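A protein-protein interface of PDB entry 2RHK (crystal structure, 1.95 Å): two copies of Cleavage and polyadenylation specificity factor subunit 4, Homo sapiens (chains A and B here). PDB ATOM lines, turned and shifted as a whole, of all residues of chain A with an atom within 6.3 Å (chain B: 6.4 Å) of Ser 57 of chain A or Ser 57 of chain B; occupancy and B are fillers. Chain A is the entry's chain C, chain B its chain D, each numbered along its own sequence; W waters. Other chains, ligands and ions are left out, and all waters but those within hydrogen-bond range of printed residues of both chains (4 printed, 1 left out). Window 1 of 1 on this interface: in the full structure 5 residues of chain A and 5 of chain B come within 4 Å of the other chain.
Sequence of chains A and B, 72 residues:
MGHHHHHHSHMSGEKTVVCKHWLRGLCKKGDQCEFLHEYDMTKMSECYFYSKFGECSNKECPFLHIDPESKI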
ATOM      1  N   PHE A  49     -17.576   8.522  17.993  1.00  0.00           N
ATOM      2  CA  PHE A  49     -17.484   7.508  16.946  1.00  0.00           C
ATOM      3  C   PHE A  49     -18.330   6.269  17.207  1.00  0.00           C
ATOM      4  O   PHE A  49     -19.003   5.773  16.299  1.00  0.00           O
ATOM      5  CB  PHE A  49     -16.017   7.154  16.714  1.00  0.00           C
ATOM      6  CG  PHE A  49     -15.230   8.291  16.122  1.00  0.00           C
ATOM      7  CD1 PHE A  49     -15.397   8.636  14.788  1.00  0.00           C
ATOM      8  CD2 PHE A  49     -14.399   9.073  16.919  1.00  0.00           C
ATOM      9  CE1 PHE A  49     -14.750   9.756  14.254  1.00  0.00           C
ATOM     10  CE2 PHE A  49     -13.749  10.195  16.399  1.00  0.00           C
ATOM     11  CZ  PHE A  49     -13.926  10.536  15.064  1.00  0.00           C
ATOM     12  N   GLU A  55     -19.069   1.896  16.215  1.00  0.00           N
ATOM     13  CA  GLU A  55     -17.813   1.224  16.476  1.00  0.00           C
ATOM     14  C   GLU A  55     -16.705   2.239  16.693  1.00  0.00           C
ATOM     15  O   GLU A  55     -16.826   3.399  16.299  1.00  0.00           O
ATOM     16  CB  GLU A  55     -17.464   0.307  15.319  1.00  0.00           C
ATOM     17  CG  GLU A  55     -17.452   1.015  14.008  1.00  0.00           C
ATOM     18  CD  GLU A  55     -16.695   0.237  12.976  1.00  0.00           C
ATOM     19  OE1 GLU A  55     -17.250  -0.741  12.435  1.00  0.00           O
ATOM     20  OE2 GLU A  55     -15.528   0.596  12.727  1.00  0.00           O
ATOM     21  N   CYS A  56     -15.616   1.779  17.293  1.00  0.00           N
ATOM     22  CA  CYS A  56     -14.497   2.644  17.637  1.00  0.00           C
ATOM     23  C   CYS A  56     -13.197   1.862  17.513  1.00  0.00           C
ATOM     24  O   CYS A  56     -13.128   0.701  17.917  1.00  0.00           O
ATOM     25  CB  CYS A  56     -14.718   3.131  19.073  1.00  0.00           C
ATOM     26  SG  CYS A  56     -13.378   4.044  19.803  1.00  0.00           S
ATOM     27  N   SER A  57     -12.165   2.495  16.956  1.00  0.00           N
ATOM     28  CA  SER A  57     -10.878   1.821  16.744  1.00  0.00           C
ATOM     29  C   SER A  57      -9.919   1.776  17.924  1.00  0.00           C
ATOM     30  O   SER A  57      -8.884   1.125  17.846  1.00  0.00           O
ATOM     31  CB  SER A  57     -10.138   2.468  15.561  1.00  0.00           C
ATOM     32  OG  SER A  57     -10.925   2.442  14.384  1.00  0.00           O
ATOM     33  N   ASN A  58     -10.240   2.466  19.013  1.00  0.00           N
ATOM     34  CA  ASN A  58      -9.334   2.491  20.156  1.00  0.00           C
ATOM     35  C   ASN A  58      -9.638   1.390  21.161  1.00  0.00           C
ATOM     36  O   ASN A  58     -10.619   1.476  21.897  1.00  0.00           O
ATOM     37  CB  ASN A  58      -9.421   3.856  20.846  1.00  0.00           C
ATOM     38  CG  ASN A  58      -8.341   4.059  21.887  1.00  0.00           C
ATOM     39  OD1 ASN A  58      -7.583   3.142  22.200  1.00  0.00           O
ATOM     40  ND2 ASN A  58      -8.265   5.274  22.431  1.00  0.00           N
ATOM     41  N   LYS A  59      -8.790   0.368  21.202  1.00  0.00           N
ATOM     42  CA  LYS A  59      -8.983  -0.738  22.140  1.00  0.00           C
ATOM     43  C   LYS A  59      -9.049  -0.203  23.566  1.00  0.00           C
ATOM     44  O   LYS A  59      -9.666  -0.812  24.436  1.00  0.00           O
ATOM     45  CB  LYS A  59      -7.826  -1.736  22.049  1.00  0.00           C
ATOM     46  CG  LYS A  59      -7.729  -2.495  20.734  1.00  0.00           C
ATOM     47  CD  LYS A  59      -6.563  -3.475  20.775  1.00  0.00           C
ATOM     48  CE  LYS A  59      -6.292  -4.068  19.402  1.00  0.00           C
ATOM     49  NZ  LYS A  59      -4.940  -4.717  19.356  1.00  0.00           N
ATOM     50  N   GLU A  60      -8.405   0.938  23.797  1.00  0.00           N
ATOM     51  CA  GLU A  60      -8.382   1.548  25.121  1.00  0.00           C
ATOM     52  C   GLU A  60      -9.275   2.782  25.183  1.00  0.00           C
ATOM     53  O   GLU A  60      -9.041   3.668  26.009  1.00  0.00           O
ATOM     54  CB  GLU A  60      -6.948   1.956  25.502  1.00  0.00           C
ATOM     55  CG  GLU A  60      -6.031   0.833  25.974  1.00  0.00           C
ATOM     56  CD  GLU A  60      -5.709  -0.184  24.895  1.00  0.00           C
ATOM     57  OE1 GLU A  60      -5.085   0.184  23.875  1.00  0.00           O
ATOM     58  OE2 GLU A  60      -6.079  -1.366  25.076  1.00  0.00           O
ATOM     59  N   PHE B  49       4.780  -0.011  17.548  1.00  0.00           N
ATOM     60  CA  PHE B  49       4.285  -0.182  18.913  1.00  0.00           C
ATOM     61  C   PHE B  49       4.127  -1.633  19.326  1.00  0.00           C
ATOM     62  O   PHE B  49       4.475  -2.002  20.450  1.00  0.00           O
ATOM     63  CB  PHE B  49       2.986   0.599  19.087  1.00  0.00           C
ATOM     64  CG  PHE B  49       3.186   2.079  18.997  1.00  0.00           C
ATOM     65  CD1 PHE B  49       3.708   2.785  20.071  1.00  0.00           C
ATOM     66  CD2 PHE B  49       2.938   2.757  17.804  1.00  0.00           C
ATOM     67  CE1 PHE B  49       3.991   4.154  19.958  1.00  0.00           C
ATOM     68  CE2 PHE B  49       3.215   4.118  17.686  1.00  0.00           C
ATOM     69  CZ  PHE B  49       3.743   4.817  18.766  1.00  0.00           C
ATOM     70  N   GLU B  55       2.105  -4.448  22.364  1.00  0.00           N
ATOM     71  CA  GLU B  55       0.671  -4.198  22.284  1.00  0.00           C
ATOM     72  C   GLU B  55       0.421  -3.019  21.345  1.00  0.00           C
ATOM     73  O   GLU B  55       1.319  -2.211  21.105  1.00  0.00           O
ATOM     74  CB  GLU B  55       0.091  -3.891  23.684  1.00  0.00           C
ATOM     75  CG  GLU B  55       0.388  -2.483  24.182  1.00  0.00           C
ATOM     76  CD  GLU B  55      -0.234  -2.180  25.542  1.00  0.00           C
ATOM     77  OE1 GLU B  55      -1.470  -2.304  25.684  1.00  0.00           O
ATOM     78  OE2 GLU B  55       0.521  -1.808  26.466  1.00  0.00           O
ATOM     79  N   CYS B  56      -0.799  -2.935  20.819  1.00  0.00           N
ATOM     80  CA  CYS B  56      -1.181  -1.866  19.895  1.00  0.00           C
ATOM     81  C   CYS B  56      -2.649  -1.522  20.118  1.00  0.00           C
ATOM     82  O   CYS B  56      -3.498  -2.412  20.144  1.00  0.00           O
ATOM     83  CB  CYS B  56      -0.958  -2.318  18.442  1.00  0.00           C
ATOM     84  SG  CYS B  56      -1.440  -1.075  17.218  1.00  0.00           S
ATOM     85  N   SER B  57      -2.941  -0.235  20.273  1.00  0.00           N
ATOM     86  CA  SER B  57      -4.310   0.231  20.551  1.00  0.00           C
ATOM     87  C   SER B  57      -5.268   0.294  19.363  1.00  0.00           C
ATOM     88  O   SER B  57      -6.475   0.456  19.547  1.00  0.00           O
ATOM     89  CB  SER B  57      -4.274   1.631  21.175  1.00  0.00           C
ATOM     90  OG  SER B  57      -3.517   1.671  22.361  1.00  0.00           O
ATOM     91  N   ASN B  58      -4.746   0.177  18.150  1.00  0.00           N
ATOM     92  CA  ASN B  58      -5.602   0.285  16.975  1.00  0.00           C
ATOM     93  C   ASN B  58      -6.198  -1.059  16.604  1.00  0.00           C
ATOM     94  O   ASN B  58      -5.481  -1.943  16.144  1.00  0.00           O
ATOM     95  CB  ASN B  58      -4.784   0.855  15.807  1.00  0.00           C
ATOM     96  CG  ASN B  58      -5.638   1.188  14.596  1.00  0.00           C
ATOM     97  OD1 ASN B  58      -6.858   1.015  14.609  1.00  0.00           O
ATOM     98  ND2 ASN B  58      -4.998   1.679  13.543  1.00  0.00           N
ATOM     99  N   LYS B  59      -7.508  -1.217  16.797  1.00  0.00           N
ATOM    100  CA  LYS B  59      -8.168  -2.481  16.458  1.00  0.00           C
ATOM    101  C   LYS B  59      -8.017  -2.775  14.972  1.00  0.00           C
ATOM    102  O   LYS B  59      -8.062  -3.925  14.556  1.00  0.00           O
ATOM    103  CB  LYS B  59      -9.668  -2.440  16.773  1.00  0.00           C
ATOM    104  CG  LYS B  59     -10.030  -2.176  18.216  1.00  0.00           C
ATOM    105  CD  LYS B  59     -11.538  -2.220  18.390  1.00  0.00           C
ATOM    106  CE  LYS B  59     -11.954  -1.676  19.740  1.00  0.00           C
ATOM    107  NZ  LYS B  59     -13.422  -1.438  19.805  1.00  0.00           N
ATOM    108  N   GLU B  60      -7.857  -1.724  14.173  1.00  0.00           N
ATOM    109  CA  GLU B  60      -7.713  -1.899  12.731  1.00  0.00           C
ATOM    110  C   GLU B  60      -6.291  -1.621  12.269  1.00  0.00           C
ATOM    111  O   GLU B  60      -6.089  -1.242  11.121  1.00  0.00           O
ATOM    112  CB  GLU B  60      -8.656  -0.962  11.953  1.00  0.00           C
ATOM    113  CG  GLU B  60     -10.138  -1.334  11.956  1.00  0.00           C
ATOM    114  CD  GLU B  60     -10.826  -1.018  13.265  1.00  0.00           C
ATOM    115  OE1 GLU B  60     -10.730   0.137  13.725  1.00  0.00           O
ATOM    116  OE2 GLU B  60     -11.471  -1.924  13.833  1.00  0.00           O
ATOM    117  N   HIS B  65       1.853  -7.299  13.192  1.00  0.00           N
ATOM    118  CA  HIS B  65       1.988  -7.538  14.620  1.00  0.00           C
ATOM    119  C   HIS B  65       2.748  -8.849  14.787  1.00  0.00           C
ATOM    120  O   HIS B  65       2.159  -9.928  14.866  1.00  0.00           O
ATOM    121  CB  HIS B  65       0.612  -7.606  15.292  1.00  0.00           C
ATOM    122  CG  HIS B  65      -0.026  -6.264  15.498  1.00  0.00           C
ATOM    123  ND1 HIS B  65      -1.246  -6.109  16.121  1.00  0.00           N
ATOM    124  CD2 HIS B  65       0.394  -5.014  15.180  1.00  0.00           C
ATOM    125  CE1 HIS B  65      -1.552  -4.825  16.179  1.00  0.00           C
ATOM    126  NE2 HIS B  65      -0.574  -4.138  15.618  1.00  0.00           N
HETATM  127  O   HOH W   1      -2.421  -5.619  21.027  1.00  0.00           O
HETATM  128  O   HOH W   2     -12.980   0.038  22.009  1.00  0.00           O
HETATM  129  O   HOH W   3     -16.052  -1.057  18.310  1.00  0.00           O
HETATM  130  O   HOH W   4      -4.638  -4.472  16.741  1.00  0.00           O
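The backbone carbonyl oxygen (O) of Cys 56 of chain A is in hydrogen-bond range of the side-chain amino group (NZ) of Lys 59 of chain B (2.9 Å). N of Lys 59 of chain B is in hydrogen-bond range of O of Ser 57 of chain A (2.9 Å). OG of Ser 57 of chain A lies within hydrogen-bond range of OE1 of Glu 60 of chain B, at 2.4 Å. The side-chain amino group (NZ) of Lys 59 of chain A sits at hydrogen-bond distance from the backbone carbonyl oxygen (O) of Cys 56 of chain B (2.8 Å). The backbone carbonyl oxygen of Ser 57 of chain B is in hydrogen-bond range of the backbone NH of Lys 59 of chain A (2.8 Å). The side-chain carboxylate (OE1) of Glu 60 of chain A lies within hydrogen-bond range of the side-chain hydroxyl (OG) of Ser 57 of chain B, at 2.6 Å. The backbone carbonyl oxygen (O) of Ser 57 of chain B sits close to the backbone carbonyl oxygen (O) of Ser 57 of chain A.
The side-chain sulfur of Cys 56 of chain A sits close to the backbone NH of Asn 58 of chain A (3.6 Å). The backbone NH of Glu 60 of chain A is in hydrogen-bond range of the side-chain amide oxygen of Asn 58 of chain A. SG of Cys 56 of chain B sits close to N of Asn 58 of chain B. OD1 of Asn 58 of chain B lies within hydrogen-bond range of N of Glu 60 of chain B.
Among the printed residues, merely in contact across the chains: Ser 57 of chain A with Asn 58 of chain B (3.5 Å), Asn 58 of chain A with Ser 57 of chain B (3.6 Å), Lys 59 of chain A with Asn 58 of chain B (3.97 Å) and Lys 59 of chain A with Lys 59 of chain B (3.4 Å).
Ser 57 of chain A touches just these residues of chain B: Ser 57, Asn 58, Lys 59 and Glu 60. Printed residues of chain B within 4 Å of Asn 58 of chain A: Ser 57. Of the printed residues of chain B, Lys 59 of chain A touches Cys 56 (2.8 Å), Ser 57 (2.8 Å), Asn 58 (3.97 Å) and Lys 59 (3.4 Å). Phe 49 of chain B touches none of the printed residues of chain A. Printed residues of chain A within 4 Å of Cys 56 of chain B: Lys 59 (2.8 Å). Of chain A, only Ser 57 (3.0 Å), Asn 58 (3.6 Å), Lys 59 (2.8 Å) and Glu 60 (2.6 Å) come within 4 Å of Ser 57 of chain B. The nearest printed residue of chain A that does not touch Ser 57 of chain B is Cys 56 of chain A (6.9 Å). The nearest printed residue of chain B that does not touch Glu 60 of chain A is Glu 55 of chain B (4.7 Å).
Of the 8 printed residues of chain B, 5 touch a printed residue of chain A. Of the 7 printed residues of chain A, 5 touch a printed residue of chain B. Printed residues of chain A that touch a printed residue of chain B: Cys 56, Ser 57, Asn 58, Lys 59 and Glu 60.
Ser 57 of chain A touches Asn 58 of chain B, and with the chains exchanged Asn 58 of chain A touches Ser 57 of chain B. Ser 57 of chain A touches Lys 59 of chain B, and with the chains exchanged Lys 59 of chain A touches Ser 57 of chain B. Ser 57 of chain A touches Glu 60 of chain B, and with the chains exchanged Glu 60 of chain A touches Ser 57 of chain B. Lys 59 of chain A touches Asn 58 of chain B, but with the chains exchanged Asn 58 of chain A does not touch Lys 59 of chain B (4.05 Å).
Water W4 lies within hydrogen-bond range of NZ of Lys 59 of chain A and O of Asn 58 of chain B. Water W2 lies within hydrogen-bond range of NZ of Lys 59 of chain B (2.7 Å) and O of Asn 58 of chain A (2.8 Å). Water W3 bridges the backbone NH of Cys 56 of chain A and the side-chain amino group of Lys 59 of chain B. Water W1 lies within hydrogen-bond range of the backbone NH (N) of Cys 56 of chain B (3.1 Å) and the side-chain amino group (NZ) of Lys 59 of chain A (3.2 Å).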
